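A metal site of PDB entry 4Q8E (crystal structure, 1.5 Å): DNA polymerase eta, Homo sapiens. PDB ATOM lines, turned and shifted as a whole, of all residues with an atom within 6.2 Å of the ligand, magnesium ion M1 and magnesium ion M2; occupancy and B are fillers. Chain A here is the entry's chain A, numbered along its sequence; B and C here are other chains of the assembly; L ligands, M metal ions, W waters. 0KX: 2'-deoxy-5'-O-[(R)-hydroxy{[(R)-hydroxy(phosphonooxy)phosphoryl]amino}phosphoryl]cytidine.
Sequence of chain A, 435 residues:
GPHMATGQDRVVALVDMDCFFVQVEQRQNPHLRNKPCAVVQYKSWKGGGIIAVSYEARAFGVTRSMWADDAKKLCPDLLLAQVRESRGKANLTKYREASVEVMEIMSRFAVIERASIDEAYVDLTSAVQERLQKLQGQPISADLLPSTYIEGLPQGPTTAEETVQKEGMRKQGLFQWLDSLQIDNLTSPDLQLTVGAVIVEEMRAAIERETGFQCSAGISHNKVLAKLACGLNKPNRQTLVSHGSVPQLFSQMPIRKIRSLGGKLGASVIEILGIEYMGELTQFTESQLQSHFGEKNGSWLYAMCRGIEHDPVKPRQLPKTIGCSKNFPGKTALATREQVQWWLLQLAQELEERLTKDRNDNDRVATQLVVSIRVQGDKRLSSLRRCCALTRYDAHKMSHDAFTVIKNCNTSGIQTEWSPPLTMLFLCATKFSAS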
ATOM      1  N   ASP A  16     -27.506  25.765  13.883  1.00  0.00           N
ATOM      2  CA  ASP A  16     -26.712  25.179  14.959  1.00  0.00           C
ATOM      3  C   ASP A  16     -27.115  23.721  15.164  1.00  0.00           C
ATOM      4  O   ASP A  16     -28.277  23.414  15.434  1.00  0.00           O
ATOM      5  CB  ASP A  16     -26.870  25.941  16.274  1.00  0.00           C
ATOM      6  CG  ASP A  16     -25.945  25.392  17.336  1.00  0.00           C
ATOM      7  OD1 ASP A  16     -26.285  24.372  17.889  1.00  0.00           O
ATOM      8  OD2 ASP A  16     -24.849  25.932  17.539  1.00  0.00           O
ATOM      9  N   MET A  17     -26.143  22.823  15.123  1.00  0.00           N
ATOM     10  CA  MET A  17     -26.485  21.410  15.233  1.00  0.00           C
ATOM     11  C   MET A  17     -26.997  21.069  16.618  1.00  0.00           C
ATOM     12  O   MET A  17     -26.532  21.592  17.601  1.00  0.00           O
ATOM     13  CB  MET A  17     -25.241  20.556  14.932  1.00  0.00           C
ATOM     14  CG  MET A  17     -24.630  20.854  13.544  1.00  0.00           C
ATOM     15  SD  MET A  17     -25.763  20.783  12.140  1.00  0.00           S
ATOM     16  CE  MET A  17     -26.179  19.094  12.132  1.00  0.00           C
ATOM     17  N   ASP A  18     -27.998  20.194  16.679  1.00  0.00           N
ATOM     18  CA  ASP A  18     -28.493  19.753  17.993  1.00  0.00           C
ATOM     19  C   ASP A  18     -27.529  18.756  18.611  1.00  0.00           C
ATOM     20  O   ASP A  18     -26.985  17.875  17.899  1.00  0.00           O
ATOM     21  CB  ASP A  18     -29.880  19.121  17.830  1.00  0.00           C
ATOM     22  CG  ASP A  18     -30.916  20.113  17.299  1.00  0.00           C
ATOM     23  OD1 ASP A  18     -30.759  21.320  17.552  1.00  0.00           O
ATOM     24  OD2 ASP A  18     -31.880  19.686  16.660  1.00  0.00           O
ATOM     25  N   CYS A  19     -27.311  18.882  19.923  1.00  0.00           N
ATOM     26  CA  CYS A  19     -26.384  18.011  20.703  1.00  0.00           C
ATOM     27  C   CYS A  19     -25.315  17.355  19.818  1.00  0.00           C
ATOM     28  O   CYS A  19     -25.287  16.130  19.650  1.00  0.00           O
ATOM     29  CB  CYS A  19     -27.148  16.992  21.570  1.00  0.00           C
ATOM     30  SG  CYS A  19     -28.346  15.922  20.722  1.00  0.00           S
ATOM     31  N   PHE A  20     -24.488  18.185  19.220  1.00  0.00           N
ATOM     32  CA  PHE A  20     -23.759  17.753  18.016  1.00  0.00           C
ATOM     33  C   PHE A  20     -22.896  16.514  18.232  1.00  0.00           C
ATOM     34  O   PHE A  20     -23.048  15.565  17.495  1.00  0.00           O
ATOM     35  CB  PHE A  20     -22.889  18.883  17.466  1.00  0.00           C
ATOM     36  CG  PHE A  20     -22.172  18.541  16.183  1.00  0.00           C
ATOM     37  CD1 PHE A  20     -22.856  17.947  15.111  1.00  0.00           C
ATOM     38  CD2 PHE A  20     -20.827  18.825  16.043  1.00  0.00           C
ATOM     39  CE1 PHE A  20     -22.171  17.649  13.914  1.00  0.00           C
ATOM     40  CE2 PHE A  20     -20.140  18.531  14.824  1.00  0.00           C
ATOM     41  CZ  PHE A  20     -20.830  17.950  13.799  1.00  0.00           C
ATOM     42  N   PHE A  21     -22.000  16.524  19.213  1.00  0.00           N
ATOM     43  CA  PHE A  21     -21.075  15.381  19.322  1.00  0.00           C
ATOM     44  C   PHE A  21     -21.861  14.111  19.653  1.00  0.00           C
ATOM     45  O   PHE A  21     -21.484  13.024  19.254  1.00  0.00           O
ATOM     46  CB  PHE A  21     -20.006  15.585  20.408  1.00  0.00           C
ATOM     47  CG  PHE A  21     -18.937  16.601  20.079  1.00  0.00           C
ATOM     48  CD1 PHE A  21     -19.054  17.470  18.998  1.00  0.00           C
ATOM     49  CD2 PHE A  21     -17.793  16.664  20.859  1.00  0.00           C
ATOM     50  CE1 PHE A  21     -18.035  18.417  18.730  1.00  0.00           C
ATOM     51  CE2 PHE A  21     -16.782  17.600  20.585  1.00  0.00           C
ATOM     52  CZ  PHE A  21     -16.926  18.491  19.529  1.00  0.00           C
ATOM     53  N   VAL A  22     -22.959  14.245  20.410  1.00  0.00           N
ATOM     54  CA  VAL A  22     -23.828  13.101  20.678  1.00  0.00           C
ATOM     55  C   VAL A  22     -24.432  12.575  19.352  1.00  0.00           C
ATOM     56  O   VAL A  22     -24.449  11.371  19.117  1.00  0.00           O
ATOM     57  CB  VAL A  22     -24.946  13.485  21.682  1.00  0.00           C
ATOM     58  CG1 VAL A  22     -26.095  12.451  21.648  1.00  0.00           C
ATOM     59  CG2 VAL A  22     -24.359  13.629  23.073  1.00  0.00           C
ATOM     60  N   GLN A  41     -14.842  13.026  27.890  1.00  0.00           N
ATOM     61  CA  GLN A  41     -13.391  13.052  27.677  1.00  0.00           C
ATOM     62  C   GLN A  41     -12.696  12.526  28.934  1.00  0.00           C
ATOM     63  O   GLN A  41     -13.008  12.979  30.034  1.00  0.00           O
ATOM     64  CB  GLN A  41     -12.892  14.475  27.412  1.00  0.00           C
ATOM     65  CG  GLN A  41     -13.386  15.133  26.144  1.00  0.00           C
ATOM     66  CD  GLN A  41     -12.658  16.441  25.826  1.00  0.00           C
ATOM     67  OE1 GLN A  41     -12.154  16.612  24.710  1.00  0.00           O
ATOM     68  NE2 GLN A  41     -12.610  17.360  26.790  1.00  0.00           N
ATOM     69  N   ILE A  51     -18.992  16.554  27.777  1.00  0.00           N
ATOM     70  CA  ILE A  51     -18.922  17.727  26.916  1.00  0.00           C
ATOM     71  C   ILE A  51     -20.147  17.901  26.008  1.00  0.00           C
ATOM     72  O   ILE A  51     -20.298  18.941  25.378  1.00  0.00           O
ATOM     73  CB  ILE A  51     -17.611  17.775  26.096  1.00  0.00           C
ATOM     74  CG1 ILE A  51     -17.475  16.598  25.103  1.00  0.00           C
ATOM     75  CG2 ILE A  51     -16.428  17.809  27.077  1.00  0.00           C
ATOM     76  CD1 ILE A  51     -16.277  16.786  24.149  1.00  0.00           C
ATOM     77  N   ALA A  52     -21.020  16.894  25.933  1.00  0.00           N
ATOM     78  CA  ALA A  52     -22.261  16.987  25.149  1.00  0.00           C
ATOM     79  C   ALA A  52     -23.263  16.007  25.697  1.00  0.00           C
ATOM     80  O   ALA A  52     -22.877  14.946  26.206  1.00  0.00           O
ATOM     81  CB  ALA A  52     -22.008  16.740  23.646  1.00  0.00           C
ATOM     82  N   VAL A  53     -24.546  16.361  25.602  1.00  0.00           N
ATOM     83  CA  VAL A  53     -25.638  15.652  26.293  1.00  0.00           C
ATOM     84  C   VAL A  53     -26.874  15.575  25.413  1.00  0.00           C
ATOM     85  O   VAL A  53     -27.350  16.608  24.907  1.00  0.00           O
ATOM     86  CB  VAL A  53     -26.009  16.382  27.623  1.00  0.00           C
ATOM     87  CG1 VAL A  53     -26.934  15.533  28.455  1.00  0.00           C
ATOM     88  CG2 VAL A  53     -24.772  16.692  28.454  1.00  0.00           C
ATOM     89  N   TYR A  55     -30.827  15.180  24.427  1.00  0.00           N
ATOM     90  CA  TYR A  55     -31.988  15.804  25.033  1.00  0.00           C
ATOM     91  C   TYR A  55     -32.684  14.856  26.012  1.00  0.00           C
ATOM     92  O   TYR A  55     -33.225  15.318  27.024  1.00  0.00           O
ATOM     93  CB  TYR A  55     -32.941  16.357  23.979  1.00  0.00           C
ATOM     94  CG  TYR A  55     -32.411  17.660  23.422  1.00  0.00           C
ATOM     95  CD1 TYR A  55     -31.401  17.682  22.444  1.00  0.00           C
ATOM     96  CD2 TYR A  55     -32.817  18.868  23.950  1.00  0.00           C
ATOM     97  CE1 TYR A  55     -30.854  18.881  22.001  1.00  0.00           C
ATOM     98  CE2 TYR A  55     -32.288  20.064  23.497  1.00  0.00           C
ATOM     99  CZ  TYR A  55     -31.313  20.080  22.521  1.00  0.00           C
ATOM    100  OH  TYR A  55     -30.780  21.275  22.081  1.00  0.00           O
ATOM    101  N   ARG A  58     -30.750  15.315  29.133  1.00  0.00           N
ATOM    102  CA  ARG A  58     -30.980  16.630  29.735  1.00  0.00           C
ATOM    103  C   ARG A  58     -32.236  16.667  30.605  1.00  0.00           C
ATOM    104  O   ARG A  58     -32.271  17.414  31.588  1.00  0.00           O
ATOM    105  CB  ARG A  58     -31.059  17.738  28.684  1.00  0.00           C
ATOM    106  CG  ARG A  58     -29.790  17.945  27.925  1.00  0.00           C
ATOM    107  CD  ARG A  58     -29.981  18.993  26.857  1.00  0.00           C
ATOM    108  NE  ARG A  58     -28.948  18.883  25.825  1.00  0.00           N
ATOM    109  CZ  ARG A  58     -28.616  19.801  24.942  1.00  0.00           C
ATOM    110  NH1 ARG A  58     -29.184  20.996  24.948  1.00  0.00           N
ATOM    111  NH2 ARG A  58     -27.646  19.517  24.056  1.00  0.00           N
ATOM    112  N   ARG A  64     -23.437  19.518  30.431  1.00  0.00           N
ATOM    113  CA  ARG A  64     -22.030  19.760  30.152  1.00  0.00           C
ATOM    114  C   ARG A  64     -21.265  20.170  31.422  1.00  0.00           C
ATOM    115  O   ARG A  64     -21.820  20.797  32.326  1.00  0.00           O
ATOM    116  CB  ARG A  64     -21.987  20.855  29.071  1.00  0.00           C
ATOM    117  CG  ARG A  64     -20.670  21.629  28.984  1.00  0.00           C
ATOM    118  CD  ARG A  64     -20.610  22.426  27.691  1.00  0.00           C
ATOM    119  NE  ARG A  64     -21.028  21.578  26.588  1.00  0.00           N
ATOM    120  CZ  ARG A  64     -21.930  21.907  25.672  1.00  0.00           C
ATOM    121  NH1 ARG A  64     -22.507  23.101  25.672  1.00  0.00           N
ATOM    122  NH2 ARG A  64     -22.242  21.027  24.736  1.00  0.00           N
ATOM    123  N   SER A 116     -18.401  28.045  14.521  1.00  0.00           N
ATOM    124  CA  SER A 116     -17.891  27.100  15.497  1.00  0.00           C
ATOM    125  C   SER A 116     -17.908  25.740  14.808  1.00  0.00           C
ATOM    126  O   SER A 116     -18.307  25.629  13.667  1.00  0.00           O
ATOM    127  CB  SER A 116     -18.756  27.019  16.739  1.00  0.00           C
ATOM    128  OG  SER A 116     -19.943  26.261  16.494  1.00  0.00           O
ATOM    129  N   ILE A 117     -17.508  24.705  15.528  1.00  0.00           N
ATOM    130  CA  ILE A 117     -17.536  23.369  14.954  1.00  0.00           C
ATOM    131  C   ILE A 117     -18.950  22.954  14.514  1.00  0.00           C
ATOM    132  O   ILE A 117     -19.092  22.119  13.635  1.00  0.00           O
ATOM    133  CB  ILE A 117     -16.924  22.341  15.931  1.00  0.00           C
ATOM    134  CG1 ILE A 117     -16.452  21.093  15.175  1.00  0.00           C
ATOM    135  CG2 ILE A 117     -17.899  21.999  17.052  1.00  0.00           C
ATOM    136  CD1 ILE A 117     -15.563  20.206  16.022  1.00  0.00           C
ATOM    137  N   ASP A 118     -19.984  23.528  15.131  1.00  0.00           N
ATOM    138  CA  ASP A 118     -21.334  23.081  14.788  1.00  0.00           C
ATOM    139  C   ASP A 118     -22.313  24.176  14.417  1.00  0.00           C
ATOM    140  O   ASP A 118     -23.531  23.949  14.384  1.00  0.00           O
ATOM    141  CB  ASP A 118     -21.910  22.199  15.906  1.00  0.00           C
ATOM    142  CG  ASP A 118     -22.652  23.011  16.937  1.00  0.00           C
ATOM    143  OD1 ASP A 118     -22.227  24.165  17.278  1.00  0.00           O
ATOM    144  OD2 ASP A 118     -23.696  22.497  17.385  1.00  0.00           O
ATOM    145  N   GLU A 119     -21.797  25.338  14.053  1.00  0.00           N
ATOM    146  CA  GLU A 119     -22.732  26.333  13.566  1.00  0.00           C
ATOM    147  C   GLU A 119     -22.146  27.274  12.560  1.00  0.00           C
ATOM    148  O   GLU A 119     -20.922  27.453  12.491  1.00  0.00           O
ATOM    149  CB  GLU A 119     -23.332  27.106  14.700  1.00  0.00           C
ATOM    150  CG  GLU A 119     -22.406  27.970  15.398  1.00  0.00           C
ATOM    151  CD  GLU A 119     -22.786  28.106  16.863  1.00  0.00           C
ATOM    152  OE1 GLU A 119     -23.398  29.123  17.221  1.00  0.00           O
ATOM    153  OE2 GLU A 119     -22.486  27.179  17.635  1.00  0.00           O
ATOM    154  N   LYS A 227     -28.998  34.273  16.022  1.00  0.00           N
ATOM    155  CA  LYS A 227     -28.456  33.361  17.035  1.00  0.00           C
ATOM    156  C   LYS A 227     -29.447  33.227  18.183  1.00  0.00           C
ATOM    157  O   LYS A 227     -29.686  32.116  18.641  1.00  0.00           O
ATOM    158  CB  LYS A 227     -27.103  33.887  17.561  1.00  0.00           C
ATOM    159  CG  LYS A 227     -26.490  33.074  18.694  1.00  0.00           C
ATOM    160  CD  LYS A 227     -26.294  31.590  18.324  1.00  0.00           C
ATOM    161  CE  LYS A 227     -25.419  30.870  19.366  1.00  0.00           C
ATOM    162  NZ  LYS A 227     -25.383  29.382  19.176  1.00  0.00           N
ATOM    163  N   LYS A 234     -35.116  25.171  19.916  1.00  0.00           N
ATOM    164  CA  LYS A 234     -34.256  23.999  19.843  1.00  0.00           C
ATOM    165  C   LYS A 234     -34.828  22.891  20.736  1.00  0.00           C
ATOM    166  O   LYS A 234     -35.279  23.201  21.865  1.00  0.00           O
ATOM    167  CB  LYS A 234     -32.879  24.455  20.319  1.00  0.00           C
ATOM    168  CG  LYS A 234     -31.697  23.676  19.828  1.00  0.00           C
ATOM    169  CD  LYS A 234     -30.403  24.306  20.335  1.00  0.00           C
ATOM    170  CE  LYS A 234     -29.437  24.561  19.165  1.00  0.00           C
ATOM    171  NZ  LYS A 234     -29.040  23.281  18.465  1.00  0.00           N
ATOM    172  N   PRO A 235     -34.805  21.607  20.307  1.00  0.00           N
ATOM    173  CA  PRO A 235     -34.129  21.061  19.116  1.00  0.00           C
ATOM    174  C   PRO A 235     -35.051  20.803  17.947  1.00  0.00           C
ATOM    175  O   PRO A 235     -36.286  20.769  18.066  1.00  0.00           O
ATOM    176  CB  PRO A 235     -33.611  19.698  19.615  1.00  0.00           C
ATOM    177  CG  PRO A 235     -34.677  19.254  20.592  1.00  0.00           C
ATOM    178  CD  PRO A 235     -35.277  20.509  21.187  1.00  0.00           C
ATOM    179  P    DG B   8     -21.909  30.875  21.426  1.00  0.00           P
ATOM    180  OP1  DG B   8     -21.647  31.817  20.337  1.00  0.00           O
ATOM    181  OP2  DG B   8     -23.310  30.553  21.771  1.00  0.00           O
ATOM    182  O5'  DG B   8     -21.128  29.499  21.227  1.00  0.00           O
ATOM    183  C5'  DG B   8     -20.953  29.034  19.945  1.00  0.00           C
ATOM    184  C4'  DG B   8     -20.176  27.732  19.959  1.00  0.00           C
ATOM    185  O4'  DG B   8     -18.952  27.795  20.702  1.00  0.00           O
ATOM    186  C3'  DG B   8     -20.868  26.469  20.448  1.00  0.00           C
ATOM    187  O3'  DG B   8     -20.933  25.620  19.398  1.00  0.00           O
ATOM    188  C2'  DG B   8     -19.952  25.851  21.478  1.00  0.00           C
ATOM    189  C1'  DG B   8     -18.624  26.528  21.211  1.00  0.00           C
ATOM    190  N9   DG B   8     -17.900  26.717  22.455  1.00  0.00           N
ATOM    191  C8   DG B   8     -18.167  27.635  23.444  1.00  0.00           C
ATOM    192  N7   DG B   8     -17.361  27.552  24.459  1.00  0.00           N
ATOM    193  C5   DG B   8     -16.481  26.532  24.118  1.00  0.00           C
ATOM    194  C6   DG B   8     -15.373  25.993  24.818  1.00  0.00           C
ATOM    195  O6   DG B   8     -14.914  26.316  25.913  1.00  0.00           O
ATOM    196  N1   DG B   8     -14.776  24.948  24.107  1.00  0.00           N
ATOM    197  C2   DG B   8     -15.189  24.484  22.900  1.00  0.00           C
ATOM    198  N2   DG B   8     -14.486  23.461  22.404  1.00  0.00           N
ATOM    199  N3   DG B   8     -16.225  24.993  22.221  1.00  0.00           N
ATOM    200  C4   DG B   8     -16.804  26.006  22.887  1.00  0.00           C
ATOM    201  O3' P9G C   2      -8.454  18.563  28.717  1.00  0.00           O
ATOM    202  OP2 P9G C   2      -8.454  20.257  33.630  1.00  0.00           O
ATOM    203  P   P9G C   2      -9.761  20.964  33.466  1.00  0.00           P
ATOM    204  OP1 P9G C   2      -9.774  22.406  33.100  1.00  0.00           O
ATOM    205  O5' P9G C   2     -10.439  20.205  32.254  1.00  0.00           O
ATOM    206  C5' P9G C   2     -10.105  18.839  31.964  1.00  0.00           C
ATOM    207  C4' P9G C   2      -9.970  18.639  30.477  1.00  0.00           C
ATOM    208  O4' P9G C   2     -11.165  19.114  29.819  1.00  0.00           O
ATOM    209  C1' P9G C   2     -10.871  20.243  29.000  1.00  0.00           C
ATOM    210  C2' P9G C   2      -9.482  20.708  29.415  1.00  0.00           C
ATOM    211  C3' P9G C   2      -8.830  19.394  29.812  1.00  0.00           C
ATOM    212  N9  P9G C   2     -11.997  21.162  29.124  1.00  0.00           N
ATOM    213  C8  P9G C   2     -12.380  21.912  30.208  1.00  0.00           C
ATOM    214  N7  P9G C   2     -13.496  22.558  30.006  1.00  0.00           N
ATOM    215  C5  P9G C   2     -13.893  22.178  28.734  1.00  0.00           C
ATOM    216  C6  P9G C   2     -15.040  22.521  27.978  1.00  0.00           C
ATOM    217  O6  P9G C   2     -15.963  23.291  28.283  1.00  0.00           O
ATOM    218  N1  P9G C   2     -15.054  21.881  26.737  1.00  0.00           N
ATOM    219  C2  P9G C   2     -14.096  21.013  26.289  1.00  0.00           C
ATOM    220  N2  P9G C   2     -14.283  20.492  25.064  1.00  0.00           N
ATOM    221  N3  P9G C   2     -13.024  20.673  26.993  1.00  0.00           N
ATOM    222  C4  P9G C   2     -12.992  21.281  28.190  1.00  0.00           C
ATOM    223 PT1  P9G C   2     -14.447  23.828  31.309  1.00  0.00          PT
ATOM    224  N12 P9G C   2     -14.195  25.351  30.001  1.00  0.00           N
ATOM    225  N11 P9G C   2     -15.397  25.101  32.590  1.00  0.00           N
ATOM    226  N10 P9G C   2     -14.710  22.310  32.636  1.00  0.00           N
ATOM    227  C18 P9G C   2     -14.426  22.501  33.941  1.00  0.00           C
ATOM    228  C13 P9G C   2     -14.608  21.475  34.846  1.00  0.00           C
ATOM    229  C12 P9G C   2     -14.301  21.675  36.189  1.00  0.00           C
ATOM    230  C11 P9G C   2     -14.488  20.647  37.103  1.00  0.00           C
ATOM    231  C10 P9G C   2     -14.974  19.430  36.679  1.00  0.00           C
ATOM    232  C16 P9G C   2     -15.216  21.101  32.203  1.00  0.00           C
ATOM    233  C22 P9G C   2     -15.544  20.916  30.874  1.00  0.00           C
ATOM    234  C21 P9G C   2     -16.007  19.675  30.434  1.00  0.00           C
ATOM    235  C20 P9G C   2     -16.189  18.649  31.339  1.00  0.00           C
ATOM    236  C19 P9G C   2     -15.880  18.839  32.681  1.00  0.00           C
ATOM    237  C15 P9G C   2     -15.396  20.066  33.106  1.00  0.00           C
ATOM    238  C14 P9G C   2     -15.099  20.256  34.430  1.00  0.00           C
ATOM    239  C9  P9G C   2     -15.272  19.231  35.340  1.00  0.00           C
ATOM    240  P    DC C   3      -7.199  18.883  27.779  1.00  0.00           P
ATOM    241  OP1  DC C   3      -6.480  17.652  27.639  1.00  0.00           O
ATOM    242  OP2  DC C   3      -6.553  20.119  28.284  1.00  0.00           O
ATOM    243  O5'  DC C   3      -7.879  19.347  26.388  1.00  0.00           O
ATOM    244  C5'  DC C   3      -8.624  18.397  25.594  1.00  0.00           C
ATOM    245  C4'  DC C   3      -9.114  19.075  24.333  1.00  0.00           C
ATOM    246  O4'  DC C   3     -10.159  19.982  24.743  1.00  0.00           O
ATOM    247  C3'  DC C   3      -8.081  19.903  23.580  1.00  0.00           C
ATOM    248  O3'  DC C   3      -8.360  19.769  22.174  1.00  0.00           O
ATOM    249  C2'  DC C   3      -8.341  21.319  24.073  1.00  0.00           C
ATOM    250  C1'  DC C   3      -9.882  21.231  24.152  1.00  0.00           C
ATOM    251  N1   DC C   3     -10.527  22.288  24.945  1.00  0.00           N
ATOM    252  C2   DC C   3     -11.739  22.816  24.488  1.00  0.00           C
ATOM    253  O2   DC C   3     -12.222  22.390  23.436  1.00  0.00           O
ATOM    254  N3   DC C   3     -12.324  23.803  25.191  1.00  0.00           N
ATOM    255  C4   DC C   3     -11.788  24.237  26.331  1.00  0.00           C
ATOM    256  N4   DC C   3     -12.412  25.221  27.001  1.00  0.00           N
ATOM    257  C5   DC C   3     -10.565  23.687  26.812  1.00  0.00           C
ATOM    258  C6   DC C   3      -9.978  22.722  26.103  1.00  0.00           C
HETATM  259  PG  0KX L   1     -27.350  22.104  21.509  1.00  0.00           P
HETATM  260  O1G 0KX L   1     -27.756  22.845  22.777  1.00  0.00           O
HETATM  261  O2G 0KX L   1     -26.790  22.971  20.402  1.00  0.00           O
HETATM  262  O3G 0KX L   1     -28.485  21.280  20.986  1.00  0.00           O
HETATM  263  PB  0KX L   1     -24.668  21.053  21.507  1.00  0.00           P
HETATM  264  O1B 0KX L   1     -24.063  19.786  22.098  1.00  0.00           O
HETATM  265  O2B 0KX L   1     -24.574  21.105  20.000  1.00  0.00           O
HETATM  266  O3B 0KX L   1     -26.189  21.123  21.983  1.00  0.00           O
HETATM  267  PA  0KX L   1     -23.100  23.563  21.383  1.00  0.00           P
HETATM  268  O1A 0KX L   1     -23.771  24.046  20.176  1.00  0.00           O
HETATM  269  O2A 0KX L   1     -22.842  24.651  22.455  1.00  0.00           O
HETATM  270  N3A 0KX L   1     -24.015  22.404  22.240  1.00  0.00           N
HETATM  271  O5' 0KX L   1     -21.691  22.927  21.073  1.00  0.00           O
HETATM  272  C5' 0KX L   1     -21.420  22.093  20.001  1.00  0.00           C
HETATM  273  C4' 0KX L   1     -20.437  21.018  20.379  1.00  0.00           C
HETATM  274  O4' 0KX L   1     -19.216  21.661  20.768  1.00  0.00           O
HETATM  275  C3' 0KX L   1     -20.862  20.205  21.504  1.00  0.00           C
HETATM  276  O3' 0KX L   1     -21.665  19.084  21.068  1.00  0.00           O
HETATM  277  C2' 0KX L   1     -19.604  19.730  22.091  1.00  0.00           C
HETATM  278  C1' 0KX L   1     -18.693  20.907  21.865  1.00  0.00           C
HETATM  279  N1  0KX L   1     -18.509  21.780  22.986  1.00  0.00           N
HETATM  280  C2  0KX L   1     -17.405  21.521  23.819  1.00  0.00           C
HETATM  281  N3  0KX L   1     -17.217  22.409  24.910  1.00  0.00           N
HETATM  282  C4  0KX L   1     -18.079  23.416  25.142  1.00  0.00           C
HETATM  283  C5  0KX L   1     -19.234  23.672  24.256  1.00  0.00           C
HETATM  284  C6  0KX L   1     -19.420  22.846  23.169  1.00  0.00           C
HETATM  285  O2  0KX L   1     -16.620  20.582  23.586  1.00  0.00           O
HETATM  286  N4  0KX L   1     -17.824  24.250  26.268  1.00  0.00           N
HETATM  287 MG    MG M   1     -25.214  22.864  18.888  1.00  0.00          MG
HETATM  288 MG    MG M   2     -23.260  25.632  18.524  1.00  0.00          MG
HETATM  289  O   HOH W   1     -17.049  23.185  20.262  1.00  0.00           O
HETATM  290  O   HOH W   2     -26.048  23.130  24.872  1.00  0.00           O
HETATM  291  O   HOH W   3     -24.102  26.728  20.137  1.00  0.00           O
HETATM  292  O   HOH W   4     -24.865  19.000  24.582  1.00  0.00           O
HETATM  293  O   HOH W   5     -14.645  19.948  21.886  1.00  0.00           O
HETATM  294  O   HOH W   6     -26.622  25.809  20.917  1.00  0.00           O
HETATM  295  O   HOH W   7     -19.903  26.464  26.723  1.00  0.00           O
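Magnesium ion M1 is bound by the side-chain carboxylate (OD1) of Asp 16 (2.1 Å), the side-chain carboxylate (OD2) of Asp 118 (2.2 Å), an oxygen (O2B) of the ligand (2.2 Å), an oxygen (O2G) of the ligand (2.2 Å), the backbone carbonyl oxygen (O) of Met 17 (2.2 Å) and an oxygen (O1A) of the ligand (2.3 Å).
Magnesium ion M1 has six donor atoms within binding distance.
OD2 of Asp 16 is bound to magnesium ion M2, at 1.9 Å.
The side-chain carboxylate (OE2) of Glu 119 binds magnesium ion M2, 1.9 Å away.
Magnesium ion M2 is bound by water W3 (2.1 Å).
OD1 of Asp 118 is bound to magnesium ion M2, 2.2 Å away.
An oxygen (O1A) of the ligand binds magnesium ion M2 (2.3 Å).
O3' of DG 8 of chain B binds magnesium ion M2 (2.5 Å).
Magnesium ion M2 has six donor atoms within binding distance.
Asp 18 touches the ligand.
Ile 51 touches the ligand (O to C2', 3.5 Å).
Ala 52 touches the ligand.
Ile 117 touches the ligand.
Hydrophobic or aromatic side chains that line the ligand: Phe 20, Phe 21, Ile 51, Ala 52, Tyr 55 and Ile 117.
Within 4 Å of the ligand: Asp 16, Met 17, Asp 18, Cys 19, Phe 20, Phe 21, Ile 51, Ala 52, Tyr 55, Arg 58, Arg 64, Ile 117, Asp 118, Lys 234, DG 8 of chain B and P9G 2 of chain C.
Along chain A the residues within 4 Å of the ligand span positions 16 to 234.
The nearest printed residue that does not touch the ligand is Glu 119 (4.2 Å).
Lys 234 touches magnesium ion M1.
Four residues have an atom within 4 Å of magnesium ion M1: Asp 16, Met 17, Asp 118 and Lys 234.
Ser 116 touches magnesium ion M2.
Within 4 Å of magnesium ion M2: Asp 16, Ser 116, Asp 118, Glu 119 and DG 8 of chain B.
The side-chain hydroxyl (OH) of Tyr 55 is in hydrogen-bond range of an oxygen (O3G) of the ligand (2.5 Å).
A nitrogen (N4) of the ligand lies within hydrogen-bond range of O6 of P9G 2 of chain C.
N of Cys 19 sits at hydrogen-bond distance from O3G of the ligand, 2.9 Å away.
The side-chain amino group (NZ) of Lys 234 is in salt-bridge range of an oxygen (O3G) of the ligand, 3.3 Å away.
NH1 of Arg 58 lies within salt-bridge range of O1G of the ligand (3.2 Å).
N of Phe 20 lies within hydrogen-bond range of O1B of the ligand (3.3 Å).
N of Phe 21 sits at hydrogen-bond distance from O3' of the ligand.
An oxygen (O1B) of the ligand lies within salt-bridge range of the guanidinium group (NH2) of Arg 64 (3.4 Å).
Water W3 lies within hydrogen-bond range of NZ of Lys 227 (3.1 Å) and O2A of the ligand (3.4 Å).
Water W5 lies within hydrogen-bond range of an oxygen (O2) of the ligand and N2 of P9G 2 of chain C.
Water W1 lies within hydrogen-bond range of an oxygen (O4') of the ligand (2.7 Å) and N3 of DG 8 of chain B (2.8 Å).
The side-chain hydroxyl of Ser 116 lies close to the backbone NH of Glu 119, 3.2 Å away.
N of Asp 118 sits close to OG of Ser 116, at 3.1 Å.
The side-chain amino group (NZ) of Lys 234 lies close to the backbone carbonyl oxygen (O) of Met 17, at 3.1 Å.
O3' of DG 8 of chain B sits close to the side-chain hydroxyl (OG) of Ser 116.
OP2 of DG 8 of chain B lies within salt-bridge range of NZ of Lys 227 (3.5 Å).
N3 of P9G 2 of chain C lies within hydrogen-bond range of NE2 of Gln 41 (3.3 Å).
The side-chain carboxylate of Asp 18 lies within salt-bridge range of the side-chain amino group of Lys 234, 2.8 Å away.
O of Val 53 lies within hydrogen-bond range of NE of Arg 58 (2.9 Å).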
